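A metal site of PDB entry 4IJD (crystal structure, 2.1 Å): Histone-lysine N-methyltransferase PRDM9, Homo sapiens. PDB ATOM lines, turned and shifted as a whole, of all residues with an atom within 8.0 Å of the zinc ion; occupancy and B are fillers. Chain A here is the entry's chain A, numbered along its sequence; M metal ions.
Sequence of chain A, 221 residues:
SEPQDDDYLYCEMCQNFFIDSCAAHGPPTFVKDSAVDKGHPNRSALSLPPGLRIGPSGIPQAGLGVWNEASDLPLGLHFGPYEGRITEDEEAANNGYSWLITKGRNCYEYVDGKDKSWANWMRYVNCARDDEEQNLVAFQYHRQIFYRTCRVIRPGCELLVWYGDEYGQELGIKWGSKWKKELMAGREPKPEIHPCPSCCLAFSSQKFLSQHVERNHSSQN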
ATOM      1  N   PRO A 195      20.892 -28.200  23.730  1.00  0.00           N
ATOM      2  CA  PRO A 195      19.662 -27.423  23.585  1.00  0.00           C
ATOM      3  C   PRO A 195      18.449 -28.281  23.283  1.00  0.00           C
ATOM      4  O   PRO A 195      18.566 -29.278  22.619  1.00  0.00           O
ATOM      5  CB  PRO A 195      19.963 -26.478  22.392  1.00  0.00           C
ATOM      6  CG  PRO A 195      21.120 -27.104  21.652  1.00  0.00           C
ATOM      7  CD  PRO A 195      21.740 -28.173  22.520  1.00  0.00           C
ATOM      8  N   CYS A 196      17.295 -27.870  23.790  1.00  0.00           N
ATOM      9  CA  CYS A 196      16.013 -28.474  23.370  1.00  0.00           C
ATOM     10  C   CYS A 196      15.598 -28.030  21.961  1.00  0.00           C
ATOM     11  O   CYS A 196      15.602 -26.837  21.653  1.00  0.00           O
ATOM     12  CB  CYS A 196      14.929 -28.084  24.345  1.00  0.00           C
ATOM     13  SG  CYS A 196      13.387 -28.973  24.159  1.00  0.00           S
ATOM     14  N   PRO A 197      15.156 -28.980  21.115  1.00  0.00           N
ATOM     15  CA  PRO A 197      14.680 -28.597  19.794  1.00  0.00           C
ATOM     16  C   PRO A 197      13.272 -27.968  19.757  1.00  0.00           C
ATOM     17  O   PRO A 197      12.842 -27.533  18.690  1.00  0.00           O
ATOM     18  CB  PRO A 197      14.642 -29.937  19.067  1.00  0.00           C
ATOM     19  CG  PRO A 197      14.249 -30.905  20.142  1.00  0.00           C
ATOM     20  CD  PRO A 197      14.987 -30.425  21.349  1.00  0.00           C
ATOM     21  N   SER A 198      12.555 -27.956  20.884  1.00  0.00           N
ATOM     22  CA  SER A 198      11.113 -27.565  20.882  1.00  0.00           C
ATOM     23  C   SER A 198      10.797 -26.360  21.743  1.00  0.00           C
ATOM     24  O   SER A 198       9.621 -25.978  21.863  1.00  0.00           O
ATOM     25  CB  SER A 198      10.249 -28.718  21.383  1.00  0.00           C
ATOM     26  OG  SER A 198      10.411 -29.837  20.563  1.00  0.00           O
ATOM     27  N   CYS A 199      11.792 -25.848  22.449  1.00  0.00           N
ATOM     28  CA  CYS A 199      11.609 -24.675  23.312  1.00  0.00           C
ATOM     29  C   CYS A 199      12.981 -24.084  23.528  1.00  0.00           C
ATOM     30  O   CYS A 199      13.968 -24.575  22.963  1.00  0.00           O
ATOM     31  CB  CYS A 199      10.952 -25.022  24.643  1.00  0.00           C
ATOM     32  SG  CYS A 199      12.080 -25.630  25.935  1.00  0.00           S
ATOM     33  N   CYS A 200      13.039 -23.032  24.300  1.00  0.00           N
ATOM     34  CA  CYS A 200      14.235 -22.177  24.344  1.00  0.00           C
ATOM     35  C   CYS A 200      15.248 -22.643  25.378  1.00  0.00           C
ATOM     36  O   CYS A 200      16.308 -22.050  25.473  1.00  0.00           O
ATOM     37  CB  CYS A 200      13.837 -20.716  24.581  1.00  0.00           C
ATOM     38  SG  CYS A 200      12.740 -20.045  23.283  1.00  0.00           S
ATOM     39  N   LEU A 201      14.966 -23.734  26.087  1.00  0.00           N
ATOM     40  CA  LEU A 201      15.870 -24.218  27.141  1.00  0.00           C
ATOM     41  C   LEU A 201      17.074 -24.986  26.626  1.00  0.00           C
ATOM     42  O   LEU A 201      17.067 -25.495  25.537  1.00  0.00           O
ATOM     43  CB  LEU A 201      15.096 -25.067  28.164  1.00  0.00           C
ATOM     44  CG  LEU A 201      13.861 -24.416  28.784  1.00  0.00           C
ATOM     45  CD1 LEU A 201      13.213 -25.345  29.820  1.00  0.00           C
ATOM     46  CD2 LEU A 201      14.206 -23.065  29.404  1.00  0.00           C
ATOM     47  N   ALA A 202      18.126 -25.076  27.447  1.00  0.00           N
ATOM     48  CA  ALA A 202      19.207 -26.036  27.210  1.00  0.00           C
ATOM     49  C   ALA A 202      19.700 -26.671  28.506  1.00  0.00           C
ATOM     50  O   ALA A 202      19.479 -26.150  29.587  1.00  0.00           O
ATOM     51  CB  ALA A 202      20.342 -25.375  26.466  1.00  0.00           C
ATOM     52  N   PHE A 203      20.369 -27.815  28.379  1.00  0.00           N
ATOM     53  CA  PHE A 203      20.699 -28.639  29.511  1.00  0.00           C
ATOM     54  C   PHE A 203      22.162 -29.001  29.533  1.00  0.00           C
ATOM     55  O   PHE A 203      22.853 -28.872  28.528  1.00  0.00           O
ATOM     56  CB  PHE A 203      19.786 -29.845  29.515  1.00  0.00           C
ATOM     57  CG  PHE A 203      18.365 -29.464  29.630  1.00  0.00           C
ATOM     58  CD1 PHE A 203      17.648 -29.042  28.503  1.00  0.00           C
ATOM     59  CD2 PHE A 203      17.790 -29.345  30.878  1.00  0.00           C
ATOM     60  CE1 PHE A 203      16.351 -28.594  28.621  1.00  0.00           C
ATOM     61  CE2 PHE A 203      16.485 -28.901  31.017  1.00  0.00           C
ATOM     62  CZ  PHE A 203      15.772 -28.501  29.888  1.00  0.00           C
ATOM     63  N   LEU A 209      18.429 -33.439  29.243  1.00  0.00           N
ATOM     64  CA  LEU A 209      17.646 -33.062  28.071  1.00  0.00           C
ATOM     65  C   LEU A 209      16.533 -34.099  27.784  1.00  0.00           C
ATOM     66  O   LEU A 209      15.423 -33.711  27.461  1.00  0.00           O
ATOM     67  CB  LEU A 209      18.545 -32.819  26.838  1.00  0.00           C
ATOM     68  CG  LEU A 209      17.776 -32.707  25.495  1.00  0.00           C
ATOM     69  CD1 LEU A 209      16.890 -31.463  25.489  1.00  0.00           C
ATOM     70  CD2 LEU A 209      18.717 -32.703  24.295  1.00  0.00           C
ATOM     71  N   HIS A 212      13.772 -33.820  30.281  1.00  0.00           N
ATOM     72  CA  HIS A 212      13.010 -32.618  29.945  1.00  0.00           C
ATOM     73  C   HIS A 212      12.089 -32.848  28.781  1.00  0.00           C
ATOM     74  O   HIS A 212      10.943 -32.454  28.817  1.00  0.00           O
ATOM     75  CB  HIS A 212      13.939 -31.471  29.630  1.00  0.00           C
ATOM     76  CG  HIS A 212      13.268 -30.345  28.887  1.00  0.00           C
ATOM     77  ND1 HIS A 212      12.473 -29.428  29.503  1.00  0.00           N
ATOM     78  CD2 HIS A 212      13.282 -30.005  27.539  1.00  0.00           C
ATOM     79  CE1 HIS A 212      12.007 -28.567  28.576  1.00  0.00           C
ATOM     80  NE2 HIS A 212      12.493 -28.934  27.388  1.00  0.00           N
ATOM     81  N   VAL A 213      12.582 -33.494  27.729  1.00  0.00           N
ATOM     82  CA  VAL A 213      11.780 -33.708  26.536  1.00  0.00           C
ATOM     83  C   VAL A 213      10.598 -34.601  26.848  1.00  0.00           C
ATOM     84  O   VAL A 213       9.493 -34.337  26.420  1.00  0.00           O
ATOM     85  CB  VAL A 213      12.612 -34.272  25.382  1.00  0.00           C
ATOM     86  CG1 VAL A 213      11.738 -34.980  24.359  1.00  0.00           C
ATOM     87  CG2 VAL A 213      13.392 -33.146  24.729  1.00  0.00           C
ATOM     88  N   ASN A 216       7.995 -32.593  29.033  1.00  0.00           N
ATOM     89  CA  ASN A 216       7.448 -31.356  28.454  1.00  0.00           C
ATOM     90  C   ASN A 216       6.991 -31.398  26.997  1.00  0.00           C
ATOM     91  O   ASN A 216       6.311 -30.464  26.550  1.00  0.00           O
ATOM     92  CB  ASN A 216       8.472 -30.244  28.614  1.00  0.00           C
ATOM     93  CG  ASN A 216       8.741 -29.934  30.075  1.00  0.00           C
ATOM     94  OD1 ASN A 216       7.997 -29.189  30.684  1.00  0.00           O
ATOM     95  ND2 ASN A 216       9.775 -30.553  30.637  1.00  0.00           N
ATOM     96  N   HIS A 217       7.402 -32.392  26.223  1.00  0.00           N
ATOM     97  CA  HIS A 217       7.137 -32.310  24.771  1.00  0.00           C
ATOM     98  C   HIS A 217       6.709 -33.597  24.127  1.00  0.00           C
ATOM     99  O   HIS A 217       5.814 -33.585  23.276  1.00  0.00           O
ATOM    100  CB  HIS A 217       8.360 -31.787  24.023  1.00  0.00           C
ATOM    101  CG  HIS A 217       8.880 -30.460  24.511  1.00  0.00           C
ATOM    102  ND1 HIS A 217       8.163 -29.295  24.395  1.00  0.00           N
ATOM    103  CD2 HIS A 217      10.130 -30.085  24.977  1.00  0.00           C
ATOM    104  CE1 HIS A 217       8.906 -28.280  24.807  1.00  0.00           C
ATOM    105  NE2 HIS A 217      10.105 -28.745  25.163  1.00  0.00           N
HETATM  106 ZN    ZN M   1      11.984 -27.882  25.613  1.00  0.00          ZN
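O of His 212 lies within hydrogen-bond range of ND2 of Asn 216 (2.9 Å). The backbone NH of Leu 201 lies close to the side-chain sulfur of Cys 199 (3.5 Å). N of Cys 196 sits at hydrogen-bond distance from O of Leu 201, at 3.0 Å. SG of Cys 196 lies close to N of Ser 198, 3.5 Å away.
The zinc ion is bound by NE2 of His 217, NE2 of His 212, SG of Cys 199 and SG of Cys 196.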
